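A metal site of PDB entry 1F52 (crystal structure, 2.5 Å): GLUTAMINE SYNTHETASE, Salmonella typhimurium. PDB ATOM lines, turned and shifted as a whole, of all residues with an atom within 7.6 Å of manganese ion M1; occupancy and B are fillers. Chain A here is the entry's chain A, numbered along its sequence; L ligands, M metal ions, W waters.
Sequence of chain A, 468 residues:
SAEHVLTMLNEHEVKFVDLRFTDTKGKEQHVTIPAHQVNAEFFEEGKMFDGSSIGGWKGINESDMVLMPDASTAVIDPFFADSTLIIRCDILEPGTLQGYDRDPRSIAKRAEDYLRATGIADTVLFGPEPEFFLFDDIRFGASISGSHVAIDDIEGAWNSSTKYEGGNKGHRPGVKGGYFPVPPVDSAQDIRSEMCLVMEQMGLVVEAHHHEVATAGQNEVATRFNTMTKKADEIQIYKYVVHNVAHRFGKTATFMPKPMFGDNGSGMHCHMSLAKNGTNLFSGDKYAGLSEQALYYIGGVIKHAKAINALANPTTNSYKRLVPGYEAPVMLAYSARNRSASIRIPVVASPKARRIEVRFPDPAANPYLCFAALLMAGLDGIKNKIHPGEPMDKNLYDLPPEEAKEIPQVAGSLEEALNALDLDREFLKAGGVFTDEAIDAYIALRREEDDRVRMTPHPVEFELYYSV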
ATOM      1  N   GLU A 129     -14.219   4.367   6.633  1.00  0.00           N
ATOM      2  CA  GLU A 129     -14.202   3.499   5.458  1.00  0.00           C
ATOM      3  C   GLU A 129     -14.808   4.221   4.266  1.00  0.00           C
ATOM      4  O   GLU A 129     -15.949   3.969   3.883  1.00  0.00           O
ATOM      5  CB  GLU A 129     -15.013   2.229   5.750  1.00  0.00           C
ATOM      6  CG  GLU A 129     -14.619   1.572   7.060  1.00  0.00           C
ATOM      7  CD  GLU A 129     -15.508   0.409   7.471  1.00  0.00           C
ATOM      8  OE1 GLU A 129     -14.905  -0.629   7.797  1.00  0.00           O
ATOM      9  OE2 GLU A 129     -16.753   0.513   7.489  1.00  0.00           O
ATOM     10  N   PRO A 130     -14.052   5.143   3.683  1.00  0.00           N
ATOM     11  CA  PRO A 130     -14.619   5.853   2.544  1.00  0.00           C
ATOM     12  C   PRO A 130     -14.675   4.977   1.297  1.00  0.00           C
ATOM     13  O   PRO A 130     -13.753   4.215   1.009  1.00  0.00           O
ATOM     14  CB  PRO A 130     -13.669   7.020   2.368  1.00  0.00           C
ATOM     15  CG  PRO A 130     -12.363   6.421   2.729  1.00  0.00           C
ATOM     16  CD  PRO A 130     -12.676   5.582   3.950  1.00  0.00           C
ATOM     17  N   GLU A 131     -15.815   5.048   0.613  1.00  0.00           N
ATOM     18  CA  GLU A 131     -16.063   4.327  -0.630  1.00  0.00           C
ATOM     19  C   GLU A 131     -16.019   5.373  -1.746  1.00  0.00           C
ATOM     20  O   GLU A 131     -16.156   6.567  -1.476  1.00  0.00           O
ATOM     21  CB  GLU A 131     -17.453   3.670  -0.560  1.00  0.00           C
ATOM     22  CG  GLU A 131     -17.466   2.421   0.319  1.00  0.00           C
ATOM     23  CD  GLU A 131     -18.836   1.955   0.727  1.00  0.00           C
ATOM     24  OE1 GLU A 131     -18.927   0.806   1.228  1.00  0.00           O
ATOM     25  OE2 GLU A 131     -19.800   2.744   0.580  1.00  0.00           O
ATOM     26  N   TYR A 179     -20.595  -6.692  -5.862  1.00  0.00           N
ATOM     27  CA  TYR A 179     -19.892  -7.352  -4.746  1.00  0.00           C
ATOM     28  C   TYR A 179     -19.229  -8.685  -5.109  1.00  0.00           C
ATOM     29  O   TYR A 179     -19.803  -9.788  -5.049  1.00  0.00           O
ATOM     30  CB  TYR A 179     -20.809  -7.508  -3.530  1.00  0.00           C
ATOM     31  CG  TYR A 179     -20.282  -6.805  -2.291  1.00  0.00           C
ATOM     32  CD1 TYR A 179     -20.176  -5.422  -2.224  1.00  0.00           C
ATOM     33  CD2 TYR A 179     -19.888  -7.543  -1.183  1.00  0.00           C
ATOM     34  CE1 TYR A 179     -19.702  -4.803  -1.085  1.00  0.00           C
ATOM     35  CE2 TYR A 179     -19.418  -6.933  -0.043  1.00  0.00           C
ATOM     36  CZ  TYR A 179     -19.325  -5.558  -0.001  1.00  0.00           C
ATOM     37  OH  TYR A 179     -18.851  -4.939   1.137  1.00  0.00           O
ATOM     38  N   HIS A 210     -11.352  -3.833  -2.538  1.00  0.00           N
ATOM     39  CA  HIS A 210     -12.336  -4.631  -3.243  1.00  0.00           C
ATOM     40  C   HIS A 210     -13.309  -3.757  -4.012  1.00  0.00           C
ATOM     41  O   HIS A 210     -13.426  -2.561  -3.757  1.00  0.00           O
ATOM     42  CB  HIS A 210     -13.114  -5.490  -2.240  1.00  0.00           C
ATOM     43  CG  HIS A 210     -13.788  -4.649  -1.139  1.00  0.00           C
ATOM     44  ND1 HIS A 210     -15.084  -4.184  -1.220  1.00  0.00           N
ATOM     45  CD2 HIS A 210     -13.295  -4.186   0.034  1.00  0.00           C
ATOM     46  CE1 HIS A 210     -15.368  -3.462  -0.140  1.00  0.00           C
ATOM     47  NE2 HIS A 210     -14.290  -3.457   0.633  1.00  0.00           N
ATOM     48  N   HIS A 211     -14.006  -4.365  -4.935  1.00  0.00           N
ATOM     49  CA  HIS A 211     -15.028  -3.688  -5.709  1.00  0.00           C
ATOM     50  C   HIS A 211     -16.199  -3.532  -4.764  1.00  0.00           C
ATOM     51  O   HIS A 211     -16.390  -4.383  -3.889  1.00  0.00           O
ATOM     52  CB  HIS A 211     -15.421  -4.529  -6.893  1.00  0.00           C
ATOM     53  CG  HIS A 211     -16.249  -3.722  -7.908  1.00  0.00           C
ATOM     54  ND1 HIS A 211     -15.756  -3.371  -9.145  1.00  0.00           N
ATOM     55  CD2 HIS A 211     -17.498  -3.223  -7.844  1.00  0.00           C
ATOM     56  CE1 HIS A 211     -16.675  -2.686  -9.812  1.00  0.00           C
ATOM     57  NE2 HIS A 211     -17.746  -2.583  -9.035  1.00  0.00           N
ATOM     58  N   GLU A 212     -16.998  -2.474  -4.898  1.00  0.00           N
ATOM     59  CA  GLU A 212     -18.147  -2.343  -4.015  1.00  0.00           C
ATOM     60  C   GLU A 212     -19.402  -2.813  -4.735  1.00  0.00           C
ATOM     61  O   GLU A 212     -19.312  -3.431  -5.798  1.00  0.00           O
ATOM     62  CB  GLU A 212     -18.273  -0.932  -3.418  1.00  0.00           C
ATOM     63  CG  GLU A 212     -17.838  -0.847  -1.964  1.00  0.00           C
ATOM     64  CD  GLU A 212     -18.801  -1.465  -0.953  1.00  0.00           C
ATOM     65  OE1 GLU A 212     -19.963  -1.754  -1.346  1.00  0.00           O
ATOM     66  OE2 GLU A 212     -18.394  -1.640   0.221  1.00  0.00           O
ATOM     67  N   VAL A 213     -20.582  -2.540  -4.155  1.00  0.00           N
ATOM     68  CA  VAL A 213     -21.831  -3.042  -4.697  1.00  0.00           C
ATOM     69  C   VAL A 213     -22.301  -2.496  -6.033  1.00  0.00           C
ATOM     70  O   VAL A 213     -22.724  -3.278  -6.901  1.00  0.00           O
ATOM     71  CB  VAL A 213     -22.944  -2.796  -3.684  1.00  0.00           C
ATOM     72  CG1 VAL A 213     -24.294  -3.226  -4.253  1.00  0.00           C
ATOM     73  CG2 VAL A 213     -22.679  -3.520  -2.377  1.00  0.00           C
ATOM     74  N   GLN A 218     -17.991   1.226  -8.502  1.00  0.00           N
ATOM     75  CA  GLN A 218     -17.873   1.601  -7.094  1.00  0.00           C
ATOM     76  C   GLN A 218     -16.764   0.741  -6.538  1.00  0.00           C
ATOM     77  O   GLN A 218     -16.728  -0.464  -6.780  1.00  0.00           O
ATOM     78  CB  GLN A 218     -19.148   1.400  -6.281  1.00  0.00           C
ATOM     79  CG  GLN A 218     -19.054   2.105  -4.931  1.00  0.00           C
ATOM     80  CD  GLN A 218     -20.346   2.050  -4.139  1.00  0.00           C
ATOM     81  OE1 GLN A 218     -20.768   3.062  -3.553  1.00  0.00           O
ATOM     82  NE2 GLN A 218     -21.116   0.981  -3.990  1.00  0.00           N
ATOM     83  N   ASN A 219     -15.858   1.348  -5.774  1.00  0.00           N
ATOM     84  CA  ASN A 219     -14.732   0.610  -5.230  1.00  0.00           C
ATOM     85  C   ASN A 219     -14.400   1.069  -3.833  1.00  0.00           C
ATOM     86  O   ASN A 219     -14.939   2.088  -3.363  1.00  0.00           O
ATOM     87  CB  ASN A 219     -13.490   0.842  -6.098  1.00  0.00           C
ATOM     88  CG  ASN A 219     -13.660   0.232  -7.458  1.00  0.00           C
ATOM     89  OD1 ASN A 219     -14.102   0.894  -8.412  1.00  0.00           O
ATOM     90  ND2 ASN A 219     -13.277  -1.042  -7.574  1.00  0.00           N
ATOM     91  N   GLU A 220     -13.540   0.323  -3.142  1.00  0.00           N
ATOM     92  CA  GLU A 220     -13.138   0.696  -1.783  1.00  0.00           C
ATOM     93  C   GLU A 220     -11.757   0.197  -1.405  1.00  0.00           C
ATOM     94  O   GLU A 220     -11.409  -0.954  -1.665  1.00  0.00           O
ATOM     95  CB  GLU A 220     -14.160   0.202  -0.728  1.00  0.00           C
ATOM     96  CG  GLU A 220     -13.827   0.567   0.715  1.00  0.00           C
ATOM     97  CD  GLU A 220     -14.883   0.159   1.714  1.00  0.00           C
ATOM     98  OE1 GLU A 220     -15.936  -0.359   1.311  1.00  0.00           O
ATOM     99  OE2 GLU A 220     -14.643   0.349   2.929  1.00  0.00           O
ATOM    100  N   ASN A 264     -26.321   1.617  -5.204  1.00  0.00           N
ATOM    101  CA  ASN A 264     -25.613   2.025  -4.006  1.00  0.00           C
ATOM    102  C   ASN A 264     -25.020   3.407  -4.016  1.00  0.00           C
ATOM    103  O   ASN A 264     -24.566   3.898  -5.049  1.00  0.00           O
ATOM    104  CB  ASN A 264     -24.465   1.068  -3.788  1.00  0.00           C
ATOM    105  CG  ASN A 264     -24.528   0.406  -2.464  1.00  0.00           C
ATOM    106  OD1 ASN A 264     -23.545   0.394  -1.704  1.00  0.00           O
ATOM    107  ND2 ASN A 264     -25.671  -0.217  -2.179  1.00  0.00           N
ATOM    108  N   GLY A 267     -20.661   5.461   1.219  1.00  0.00           N
ATOM    109  CA  GLY A 267     -20.693   5.896   2.595  1.00  0.00           C
ATOM    110  C   GLY A 267     -19.303   5.919   3.181  1.00  0.00           C
ATOM    111  O   GLY A 267     -18.338   5.504   2.548  1.00  0.00           O
ATOM    112  N   HIS A 269     -18.343   4.846   6.766  1.00  0.00           N
ATOM    113  CA  HIS A 269     -18.553   4.365   8.118  1.00  0.00           C
ATOM    114  C   HIS A 269     -17.384   4.783   8.970  1.00  0.00           C
ATOM    115  O   HIS A 269     -16.236   4.763   8.525  1.00  0.00           O
ATOM    116  CB  HIS A 269     -18.577   2.847   8.139  1.00  0.00           C
ATOM    117  CG  HIS A 269     -19.676   2.232   7.353  1.00  0.00           C
ATOM    118  ND1 HIS A 269     -19.731   0.878   7.089  1.00  0.00           N
ATOM    119  CD2 HIS A 269     -20.794   2.769   6.785  1.00  0.00           C
ATOM    120  CE1 HIS A 269     -20.818   0.612   6.399  1.00  0.00           C
ATOM    121  NE2 HIS A 269     -21.479   1.738   6.205  1.00  0.00           N
ATOM    122  N   ARG A 339     -28.549  -4.418  10.549  1.00  0.00           N
ATOM    123  CA  ARG A 339     -27.911  -3.425   9.689  1.00  0.00           C
ATOM    124  C   ARG A 339     -28.913  -2.412   9.151  1.00  0.00           C
ATOM    125  O   ARG A 339     -28.912  -2.071   7.969  1.00  0.00           O
ATOM    126  CB  ARG A 339     -27.042  -4.066   8.585  1.00  0.00           C
ATOM    127  CG  ARG A 339     -25.645  -4.520   9.059  1.00  0.00           C
ATOM    128  CD  ARG A 339     -24.734  -4.869   7.878  1.00  0.00           C
ATOM    129  NE  ARG A 339     -23.479  -5.543   8.259  1.00  0.00           N
ATOM    130  CZ  ARG A 339     -22.281  -5.298   7.725  1.00  0.00           C
ATOM    131  NH1 ARG A 339     -21.189  -5.958   8.113  1.00  0.00           N
ATOM    132  NH2 ARG A 339     -22.144  -4.342   6.802  1.00  0.00           N
HETATM  133  P1  LIG L   1     -16.529  -3.149   7.765  1.00  0.00           P
HETATM  134  O1  LIG L   1     -16.886  -4.550   7.244  1.00  0.00           O
HETATM  135  O2  LIG L   1     -17.384  -2.614   8.857  1.00  0.00           O
HETATM  136  O3  LIG L   1     -16.483  -2.121   6.444  1.00  0.00           O
HETATM  137  P2  LIG L   1     -13.391  -3.314   7.550  1.00  0.00           P
HETATM  138  O4  LIG L   1     -13.015  -4.657   6.928  1.00  0.00           O
HETATM  139  O5  LIG L   1     -13.292  -2.193   6.449  1.00  0.00           O
HETATM  140  O6  LIG L   1     -14.939  -3.315   8.236  1.00  0.00           O
HETATM  141  O7  LIG L   1     -12.209  -3.031   8.674  1.00  0.00           O
HETATM  142  C1  LIG L   1     -11.484  -1.957   9.182  1.00  0.00           C
HETATM  143  C2  LIG L   1     -11.740  -0.784  10.074  1.00  0.00           C
HETATM  144  O8  LIG L   1     -11.952  -0.978  11.620  1.00  0.00           O
HETATM  145  C3  LIG L   1     -10.437  -0.125   9.990  1.00  0.00           C
HETATM  146  O9  LIG L   1     -10.691   1.226   9.696  1.00  0.00           O
HETATM  147  C4  LIG L   1      -9.850  -0.498  11.387  1.00  0.00           C
HETATM  148  O10 LIG L   1      -8.552   0.028  11.522  1.00  0.00           O
HETATM  149  C5  LIG L   1     -10.993   0.098  12.135  1.00  0.00           C
HETATM  150  N1  LIG L   1     -10.775   0.351  13.769  1.00  0.00           N
HETATM  151  C6  LIG L   1     -11.211   1.531  14.485  1.00  0.00           C
HETATM  152  N2  LIG L   1     -10.965   1.650  15.798  1.00  0.00           N
HETATM  153  C7  LIG L   1     -10.341   0.445  16.030  1.00  0.00           C
HETATM  154  C8  LIG L   1      -9.850  -0.078  17.224  1.00  0.00           C
HETATM  155  N3  LIG L   1      -9.953   0.607  18.222  1.00  0.00           N
HETATM  156  N4  LIG L   1      -9.248  -1.289  17.260  1.00  0.00           N
HETATM  157  C9  LIG L   1      -9.156  -2.013  16.113  1.00  0.00           C
HETATM  158  N5  LIG L   1      -9.584  -1.674  14.846  1.00  0.00           N
HETATM  159  C10 LIG L   1     -10.206  -0.397  14.852  1.00  0.00           C
HETATM  160 MN    MN M   1     -17.848  -0.872   1.985  1.00  0.00          MN
HETATM  161 MN    MN M   2     -18.292  -0.841   7.570  1.00  0.00          MN
HETATM  162  O   HOH W   1     -18.321  -1.539   4.993  1.00  0.00           O
HETATM  163  O   HOH W   2     -17.339   0.442   3.598  1.00  0.00           O
HETATM  164  O   HOH W   3     -19.701  -1.386   2.683  1.00  0.00           O
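The side-chain hydroxyl (OH) of Tyr 179 sits close to the side-chain carboxylate (OE2) of Glu 212 (3.5 Å). The side-chain carboxylate (OE2) of Glu 131 lies within hydrogen-bond range of the backbone NH (N) of Gly 267 (2.9 Å). N of Glu 212 lies within hydrogen-bond range of O of Gln 218 (2.8 Å). N of Glu 220 sits at hydrogen-bond distance from O of His 210 (3.0 Å).
Of the 15 residues printed, 3 come within 4 Å of manganese ion M1. The nearest printed residue that does not touch manganese ion M1 is His 210 (4.2 Å).
Manganese ion M1 is bound by OE2 of Glu 212 (2.0 Å), water W3 (2.0 Å), OE1 of Glu 220 (2.1 Å), OE1 of Glu 131 (2.1 Å) and water W2 (2.1 Å). Manganese ion M1 has five donor atoms within binding distance.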
